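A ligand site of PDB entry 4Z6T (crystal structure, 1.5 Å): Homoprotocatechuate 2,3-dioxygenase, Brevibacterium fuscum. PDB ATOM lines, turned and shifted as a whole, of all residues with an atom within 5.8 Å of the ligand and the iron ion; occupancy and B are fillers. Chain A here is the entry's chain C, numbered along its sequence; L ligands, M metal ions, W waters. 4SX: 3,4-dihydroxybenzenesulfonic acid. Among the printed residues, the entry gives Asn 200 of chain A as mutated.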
ATOM      1  N   HIS A 155     -23.626  -5.172  26.361  1.00  0.00           N
ATOM      2  CA  HIS A 155     -22.579  -4.174  26.676  1.00  0.00           C
ATOM      3  C   HIS A 155     -22.807  -3.471  27.978  1.00  0.00           C
ATOM      4  O   HIS A 155     -23.893  -3.583  28.574  1.00  0.00           O
ATOM      5  CB  HIS A 155     -22.445  -3.129  25.542  1.00  0.00           C
ATOM      6  CG  HIS A 155     -23.657  -2.278  25.315  1.00  0.00           C
ATOM      7  ND1 HIS A 155     -24.634  -2.595  24.389  1.00  0.00           N
ATOM      8  CD2 HIS A 155     -24.021  -1.097  25.853  1.00  0.00           C
ATOM      9  CE1 HIS A 155     -25.529  -1.629  24.357  1.00  0.00           C
ATOM     10  NE2 HIS A 155     -25.184  -0.712  25.229  1.00  0.00           N
ATOM     11  N   ASN A 157     -22.151   0.657  29.601  1.00  0.00           N
ATOM     12  CA  ASN A 157     -21.900   2.032  29.242  1.00  0.00           C
ATOM     13  C   ASN A 157     -21.529   2.786  30.511  1.00  0.00           C
ATOM     14  O   ASN A 157     -22.229   2.695  31.520  1.00  0.00           O
ATOM     15  CB  ASN A 157     -23.123   2.613  28.538  1.00  0.00           C
ATOM     16  CG  ASN A 157     -22.882   4.020  28.027  1.00  0.00           C
ATOM     17  OD1 ASN A 157     -22.508   4.909  28.782  1.00  0.00           O
ATOM     18  ND2 ASN A 157     -23.064   4.214  26.734  1.00  0.00           N
ATOM     19  N   ILE A 181     -19.450  10.688  19.046  1.00  0.00           N
ATOM     20  CA  ILE A 181     -20.163  11.953  18.921  1.00  0.00           C
ATOM     21  C   ILE A 181     -19.182  13.077  19.259  1.00  0.00           C
ATOM     22  O   ILE A 181     -18.588  13.085  20.351  1.00  0.00           O
ATOM     23  CB  ILE A 181     -21.393  12.040  19.843  1.00  0.00           C
ATOM     24  CG1 ILE A 181     -22.437  10.978  19.490  1.00  0.00           C
ATOM     25  CG2 ILE A 181     -22.003  13.426  19.765  1.00  0.00           C
ATOM     26  CD1 ILE A 181     -23.589  10.884  20.472  1.00  0.00           C
ATOM     27  N   TRP A 192     -18.046   4.613  21.463  1.00  0.00           N
ATOM     28  CA  TRP A 192     -18.448   3.230  21.620  1.00  0.00           C
ATOM     29  C   TRP A 192     -17.324   2.358  21.127  1.00  0.00           C
ATOM     30  O   TRP A 192     -16.669   2.676  20.120  1.00  0.00           O
ATOM     31  CB  TRP A 192     -19.684   2.968  20.782  1.00  0.00           C
ATOM     32  CG  TRP A 192     -20.951   3.532  21.330  1.00  0.00           C
ATOM     33  CD1 TRP A 192     -21.952   2.825  21.926  1.00  0.00           C
ATOM     34  CD2 TRP A 192     -21.382   4.907  21.317  1.00  0.00           C
ATOM     35  NE1 TRP A 192     -22.976   3.673  22.307  1.00  0.00           N
ATOM     36  CE2 TRP A 192     -22.659   4.953  21.925  1.00  0.00           C
ATOM     37  CE3 TRP A 192     -20.829   6.102  20.835  1.00  0.00           C
ATOM     38  CZ2 TRP A 192     -23.375   6.135  22.063  1.00  0.00           C
ATOM     39  CZ3 TRP A 192     -21.542   7.275  20.984  1.00  0.00           C
ATOM     40  CH2 TRP A 192     -22.815   7.280  21.573  1.00  0.00           C
ATOM     41  N   VAL A 199     -21.304  -3.365  17.942  1.00  0.00           N
ATOM     42  CA  VAL A 199     -20.993  -1.926  18.048  1.00  0.00           C
ATOM     43  C   VAL A 199     -20.246  -1.604  19.346  1.00  0.00           C
ATOM     44  O   VAL A 199     -19.349  -0.755  19.371  1.00  0.00           O
ATOM     45  CB  VAL A 199     -22.226  -1.041  17.809  1.00  0.00           C
ATOM     46  CG1 VAL A 199     -21.946   0.432  18.173  1.00  0.00           C
ATOM     47  CG2 VAL A 199     -22.643  -1.145  16.342  1.00  0.00           C
ATOM     48  N   ASN A 200     -20.572  -2.316  20.418  1.00  0.00           N
ATOM     49  CA  ASN A 200     -19.830  -2.125  21.669  1.00  0.00           C
ATOM     50  C   ASN A 200     -19.826  -3.291  22.627  1.00  0.00           C
ATOM     51  O   ASN A 200     -20.733  -4.111  22.620  1.00  0.00           O
ATOM     52  CB  ASN A 200     -20.191  -0.798  22.355  1.00  0.00           C
ATOM     53  CG  ASN A 200     -21.612  -0.711  22.850  1.00  0.00           C
ATOM     54  OD1 ASN A 200     -22.601  -1.146  22.196  1.00  0.00           O
ATOM     55  ND2 ASN A 200     -21.746  -0.026  23.979  1.00  0.00           N
ATOM     56  N   HIS A 214     -25.401   2.363  32.142  1.00  0.00           N
ATOM     57  CA  HIS A 214     -26.329   1.233  31.969  1.00  0.00           C
ATOM     58  C   HIS A 214     -25.647  -0.072  31.701  1.00  0.00           C
ATOM     59  O   HIS A 214     -24.466  -0.107  31.336  1.00  0.00           O
ATOM     60  CB  HIS A 214     -27.400   1.510  30.883  1.00  0.00           C
ATOM     61  CG  HIS A 214     -26.886   1.763  29.505  1.00  0.00           C
ATOM     62  ND1 HIS A 214     -26.610   3.025  29.039  1.00  0.00           N
ATOM     63  CD2 HIS A 214     -26.644   0.929  28.468  1.00  0.00           C
ATOM     64  CE1 HIS A 214     -26.240   2.961  27.766  1.00  0.00           C
ATOM     65  NE2 HIS A 214     -26.239   1.688  27.401  1.00  0.00           N
ATOM     66  N   ALA A 216     -26.630  -3.340  29.150  1.00  0.00           N
ATOM     67  CA  ALA A 216     -27.525  -3.639  28.030  1.00  0.00           C
ATOM     68  C   ALA A 216     -27.655  -5.109  27.759  1.00  0.00           C
ATOM     69  O   ALA A 216     -26.634  -5.819  27.635  1.00  0.00           O
ATOM     70  CB  ALA A 216     -27.059  -2.953  26.759  1.00  0.00           C
ATOM     71  N   ARG A 243     -36.712   6.107  28.697  1.00  0.00           N
ATOM     72  CA  ARG A 243     -36.426   6.655  27.344  1.00  0.00           C
ATOM     73  C   ARG A 243     -36.658   5.558  26.324  1.00  0.00           C
ATOM     74  O   ARG A 243     -36.300   4.412  26.568  1.00  0.00           O
ATOM     75  CB  ARG A 243     -34.980   7.154  27.260  1.00  0.00           C
ATOM     76  CG  ARG A 243     -34.519   7.537  25.865  1.00  0.00           C
ATOM     77  CD  ARG A 243     -33.139   8.140  25.764  1.00  0.00           C
ATOM     78  NE  ARG A 243     -32.794   8.187  24.336  1.00  0.00           N
ATOM     79  CZ  ARG A 243     -31.622   7.908  23.775  1.00  0.00           C
ATOM     80  NH1 ARG A 243     -30.487   7.772  24.492  1.00  0.00           N
ATOM     81  NH2 ARG A 243     -31.557   7.846  22.467  1.00  0.00           N
ATOM     82  N   HIS A 248     -31.850   3.903  17.537  1.00  0.00           N
ATOM     83  CA  HIS A 248     -30.647   4.715  17.738  1.00  0.00           C
ATOM     84  C   HIS A 248     -30.080   5.209  16.399  1.00  0.00           C
ATOM     85  O   HIS A 248     -30.217   4.555  15.378  1.00  0.00           O
ATOM     86  CB  HIS A 248     -29.532   3.895  18.408  1.00  0.00           C
ATOM     87  CG  HIS A 248     -29.665   3.688  19.866  1.00  0.00           C
ATOM     88  ND1 HIS A 248     -29.909   4.715  20.759  1.00  0.00           N
ATOM     89  CD2 HIS A 248     -29.470   2.565  20.618  1.00  0.00           C
ATOM     90  CE1 HIS A 248     -29.900   4.229  21.994  1.00  0.00           C
ATOM     91  NE2 HIS A 248     -29.619   2.937  21.933  1.00  0.00           N
ATOM     92  N   GLY A 249     -29.434   6.365  16.418  1.00  0.00           N
ATOM     93  CA  GLY A 249     -28.583   6.786  15.304  1.00  0.00           C
ATOM     94  C   GLY A 249     -27.271   6.037  15.416  1.00  0.00           C
ATOM     95  O   GLY A 249     -27.031   5.079  14.683  1.00  0.00           O
ATOM     96  N   VAL A 250     -26.461   6.437  16.377  1.00  0.00           N
ATOM     97  CA  VAL A 250     -25.326   5.621  16.767  1.00  0.00           C
ATOM     98  C   VAL A 250     -25.771   4.155  17.012  1.00  0.00           C
ATOM     99  O   VAL A 250     -26.666   3.913  17.767  1.00  0.00           O
ATOM    100  CB  VAL A 250     -24.672   6.154  18.063  1.00  0.00           C
ATOM    101  CG1 VAL A 250     -23.620   5.180  18.580  1.00  0.00           C
ATOM    102  CG2 VAL A 250     -24.060   7.529  17.824  1.00  0.00           C
ATOM    103  N   SER A 251     -25.113   3.233  16.332  1.00  0.00           N
ATOM    104  CA  SER A 251     -25.309   1.781  16.447  1.00  0.00           C
ATOM    105  C   SER A 251     -26.417   1.251  15.535  1.00  0.00           C
ATOM    106  O   SER A 251     -26.413   0.046  15.249  1.00  0.00           O
ATOM    107  CB  SER A 251     -25.560   1.269  17.872  1.00  0.00           C
ATOM    108  OG  SER A 251     -26.911   1.396  18.261  1.00  0.00           O
ATOM    109  N   TYR A 255     -33.995   0.115  20.602  1.00  0.00           N
ATOM    110  CA  TYR A 255     -33.622   0.265  22.014  1.00  0.00           C
ATOM    111  C   TYR A 255     -34.779   0.672  22.926  1.00  0.00           C
ATOM    112  O   TYR A 255     -35.803   1.228  22.510  1.00  0.00           O
ATOM    113  CB  TYR A 255     -32.505   1.287  22.134  1.00  0.00           C
ATOM    114  CG  TYR A 255     -32.941   2.739  21.988  1.00  0.00           C
ATOM    115  CD1 TYR A 255     -33.445   3.434  23.057  1.00  0.00           C
ATOM    116  CD2 TYR A 255     -32.926   3.371  20.762  1.00  0.00           C
ATOM    117  CE1 TYR A 255     -33.885   4.728  22.954  1.00  0.00           C
ATOM    118  CE2 TYR A 255     -33.360   4.687  20.629  1.00  0.00           C
ATOM    119  CZ  TYR A 255     -33.819   5.367  21.732  1.00  0.00           C
ATOM    120  OH  TYR A 255     -34.285   6.651  21.607  1.00  0.00           O
ATOM    121  N   TYR A 257     -34.755   2.074  27.354  1.00  0.00           N
ATOM    122  CA  TYR A 257     -34.143   2.194  28.686  1.00  0.00           C
ATOM    123  C   TYR A 257     -35.173   2.178  29.807  1.00  0.00           C
ATOM    124  O   TYR A 257     -36.155   2.935  29.761  1.00  0.00           O
ATOM    125  CB  TYR A 257     -33.326   3.484  28.776  1.00  0.00           C
ATOM    126  CG  TYR A 257     -32.208   3.619  27.780  1.00  0.00           C
ATOM    127  CD1 TYR A 257     -30.930   3.098  28.045  1.00  0.00           C
ATOM    128  CD2 TYR A 257     -32.418   4.229  26.556  1.00  0.00           C
ATOM    129  CE1 TYR A 257     -29.929   3.219  27.120  1.00  0.00           C
ATOM    130  CE2 TYR A 257     -31.405   4.376  25.642  1.00  0.00           C
ATOM    131  CZ  TYR A 257     -30.173   3.861  25.923  1.00  0.00           C
ATOM    132  OH  TYR A 257     -29.190   4.007  24.986  1.00  0.00           O
ATOM    133  N   GLU A 267     -30.633  -1.131  29.562  1.00  0.00           N
ATOM    134  CA  GLU A 267     -31.007  -0.964  28.153  1.00  0.00           C
ATOM    135  C   GLU A 267     -31.392  -2.333  27.588  1.00  0.00           C
ATOM    136  O   GLU A 267     -30.748  -3.330  27.852  1.00  0.00           O
ATOM    137  CB  GLU A 267     -29.864  -0.379  27.331  1.00  0.00           C
ATOM    138  CG  GLU A 267     -30.284  -0.040  25.894  1.00  0.00           C
ATOM    139  CD  GLU A 267     -29.185   0.529  25.039  1.00  0.00           C
ATOM    140  OE1 GLU A 267     -28.010   0.380  25.418  1.00  0.00           O
ATOM    141  OE2 GLU A 267     -29.503   1.079  23.968  1.00  0.00           O
ATOM    142  N   TYR A 269     -31.891  -3.921  23.697  1.00  0.00           N
ATOM    143  CA  TYR A 269     -31.169  -3.537  22.493  1.00  0.00           C
ATOM    144  C   TYR A 269     -31.267  -4.653  21.465  1.00  0.00           C
ATOM    145  O   TYR A 269     -31.200  -5.806  21.815  1.00  0.00           O
ATOM    146  CB  TYR A 269     -29.705  -3.365  22.940  1.00  0.00           C
ATOM    147  CG  TYR A 269     -28.637  -2.874  21.993  1.00  0.00           C
ATOM    148  CD1 TYR A 269     -28.314  -1.525  21.921  1.00  0.00           C
ATOM    149  CD2 TYR A 269     -27.825  -3.777  21.285  1.00  0.00           C
ATOM    150  CE1 TYR A 269     -27.244  -1.078  21.155  1.00  0.00           C
ATOM    151  CE2 TYR A 269     -26.778  -3.318  20.497  1.00  0.00           C
ATOM    152  CZ  TYR A 269     -26.486  -1.977  20.443  1.00  0.00           C
ATOM    153  OH  TYR A 269     -25.418  -1.553  19.668  1.00  0.00           O
ATOM    154  N   ARG A 292     -28.982  11.685  15.943  1.00  0.00           N
ATOM    155  CA  ARG A 292     -27.827  10.898  16.364  1.00  0.00           C
ATOM    156  C   ARG A 292     -28.123   9.871  17.465  1.00  0.00           C
ATOM    157  O   ARG A 292     -27.508   8.822  17.507  1.00  0.00           O
ATOM    158  CB  ARG A 292     -26.702  11.823  16.818  1.00  0.00           C
ATOM    159  CG  ARG A 292     -26.860  12.355  18.239  1.00  0.00           C
ATOM    160  CD  ARG A 292     -26.009  13.584  18.573  1.00  0.00           C
ATOM    161  NE  ARG A 292     -26.328  13.976  19.944  1.00  0.00           N
ATOM    162  CZ  ARG A 292     -27.437  14.615  20.303  1.00  0.00           C
ATOM    163  NH1 ARG A 292     -28.303  15.031  19.391  1.00  0.00           N
ATOM    164  NH2 ARG A 292     -27.688  14.856  21.592  1.00  0.00           N
ATOM    165  N   ARG A 293     -29.000  10.225  18.410  1.00  0.00           N
ATOM    166  CA  ARG A 293     -29.321   9.359  19.536  1.00  0.00           C
ATOM    167  C   ARG A 293     -30.637   8.626  19.354  1.00  0.00           C
ATOM    168  O   ARG A 293     -30.727   7.403  19.563  1.00  0.00           O
ATOM    169  CB  ARG A 293     -29.266  10.127  20.859  1.00  0.00           C
ATOM    170  CG  ARG A 293     -27.826  10.478  21.250  1.00  0.00           C
ATOM    171  CD  ARG A 293     -27.681  10.692  22.732  1.00  0.00           C
ATOM    172  NE  ARG A 293     -26.324  10.997  23.167  1.00  0.00           N
ATOM    173  CZ  ARG A 293     -25.435  10.135  23.659  1.00  0.00           C
ATOM    174  NH1 ARG A 293     -25.681   8.828  23.646  1.00  0.00           N
ATOM    175  NH2 ARG A 293     -24.272  10.567  24.136  1.00  0.00           N
ATOM    176  N   ASP A 294     -31.636   9.360  18.936  1.00  0.00           N
ATOM    177  CA  ASP A 294     -32.888   8.783  18.475  1.00  0.00           C
ATOM    178  C   ASP A 294     -33.050   9.208  17.008  1.00  0.00           C
ATOM    179  O   ASP A 294     -33.198  10.409  16.690  1.00  0.00           O
ATOM    180  CB  ASP A 294     -34.081   9.225  19.283  1.00  0.00           C
ATOM    181  CG  ASP A 294     -35.330   8.463  18.906  1.00  0.00           C
ATOM    182  OD1 ASP A 294     -35.495   7.358  19.447  1.00  0.00           O
ATOM    183  OD2 ASP A 294     -36.105   8.967  18.070  1.00  0.00           O
ATOM    184  N   TRP A 304     -31.569  11.087  31.420  1.00  0.00           N
ATOM    185  CA  TRP A 304     -30.673  10.191  30.688  1.00  0.00           C
ATOM    186  C   TRP A 304     -29.222  10.726  30.665  1.00  0.00           C
ATOM    187  O   TRP A 304     -28.253   9.967  30.749  1.00  0.00           O
ATOM    188  CB  TRP A 304     -31.220   9.898  29.275  1.00  0.00           C
ATOM    189  CG  TRP A 304     -30.642   8.700  28.644  1.00  0.00           C
ATOM    190  CD1 TRP A 304     -31.127   7.423  28.722  1.00  0.00           C
ATOM    191  CD2 TRP A 304     -29.412   8.609  27.873  1.00  0.00           C
ATOM    192  NE1 TRP A 304     -30.300   6.559  28.054  1.00  0.00           N
ATOM    193  CE2 TRP A 304     -29.254   7.251  27.503  1.00  0.00           C
ATOM    194  CE3 TRP A 304     -28.475   9.534  27.438  1.00  0.00           C
ATOM    195  CZ2 TRP A 304     -28.181   6.803  26.756  1.00  0.00           C
ATOM    196  CZ3 TRP A 304     -27.411   9.083  26.701  1.00  0.00           C
ATOM    197  CH2 TRP A 304     -27.271   7.741  26.349  1.00  0.00           C
HETATM  198  O11 4SX L   1     -28.679   7.110  22.093  1.00  0.00           O
HETATM  199  S9  4SX L   1     -27.430   6.610  21.232  1.00  0.00           S
HETATM  200  O12 4SX L   1     -27.864   6.419  19.826  1.00  0.00           O
HETATM  201  O10 4SX L   1     -26.342   7.591  21.350  1.00  0.00           O
HETATM  202  C4  4SX L   1     -26.879   5.069  21.800  1.00  0.00           C
HETATM  203  C3  4SX L   1     -26.899   4.854  23.188  1.00  0.00           C
HETATM  204  C5  4SX L   1     -26.418   4.084  20.925  1.00  0.00           C
HETATM  205  C6  4SX L   1     -25.986   2.857  21.397  1.00  0.00           C
HETATM  206  C1  4SX L   1     -26.115   2.594  22.756  1.00  0.00           C
HETATM  207  O7  4SX L   1     -25.805   1.372  23.279  1.00  0.00           O
HETATM  208  C2  4SX L   1     -26.545   3.603  23.674  1.00  0.00           C
HETATM  209  O8  4SX L   1     -26.785   3.247  24.967  1.00  0.00           O
HETATM  210 FE    FE M   1     -26.212   1.235  25.245  1.00  0.00          FE
HETATM  211  O   HOH W   1     -23.753   2.024  25.017  1.00  0.00           O
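The backbone carbonyl oxygen of Val 250 lies close to an oxygen (O12) of the ligand (3.5 Å).
An oxygen (O12) of the ligand lies close to the backbone carbonyl oxygen (O) of Arg 292 (3.4 Å).
Residues that only touch the ligand: Trp 192, Tyr 269, Ser 251 and Gly 249.
Hydrophobic or aromatic side chains that line the ligand: His 155, Trp 192, His 214, His 248, Val 250, Tyr 257 and Tyr 269.
Of the 21 residues printed, 3 come within 4 Å of the iron ion.
OE1 of Glu 267 is bound to the iron ion, at 2.0 Å.
O7 of the ligand binds the iron ion, 2.0 Å away.
O8 of the ligand binds the iron ion (2.1 Å).
NE2 of His 155 binds the iron ion, at 2.2 Å.
The iron ion is bound by a ring nitrogen (NE2) of His 214 (2.2 Å).
Water W1 binds the iron ion (2.6 Å).
The iron ion has six donor atoms within binding distance.
OH of Tyr 257 sits close to O8 of the ligand, at 2.5 Å.
An oxygen (O12) of the ligand lies close to the backbone carbonyl oxygen (O) of Arg 293 (3.0 Å).
An oxygen (O12) of the ligand is in hydrogen-bond range of a ring nitrogen (ND1) of His 248.
The guanidinium group (NH1) of Arg 293 is in salt-bridge range of an oxygen (O10) of the ligand (2.7 Å).
An oxygen (O11) of the ligand is in salt-bridge range of the guanidinium group of Arg 243 (3.0 Å).
ND1 of His 155 lies within hydrogen-bond range of OD1 of Asn 200, at 3.3 Å.
O of Arg 293 lies within hydrogen-bond range of ND1 of His 248 (3.1 Å).
The side-chain hydroxyl (OH) of Tyr 257 lies close to a ring nitrogen (NE2) of His 248, 3.3 Å away.
NH2 of Arg 243 sits at hydrogen-bond distance from OH of Tyr 255 (3.1 Å).
A ring nitrogen (NE2) of His 248 lies within hydrogen-bond range of the side-chain carboxylate of Glu 267, at 2.8 Å.
The backbone carbonyl oxygen (O) of Arg 293 is in hydrogen-bond range of the guanidinium group (NH2) of Arg 243, at 3.1 Å.
The backbone NH (N) of Val 250 is in hydrogen-bond range of the backbone carbonyl oxygen (O) of Arg 292 (2.8 Å).
The backbone carbonyl oxygen of Arg 292 lies close to the backbone NH of Gly 249, 3.3 Å away.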
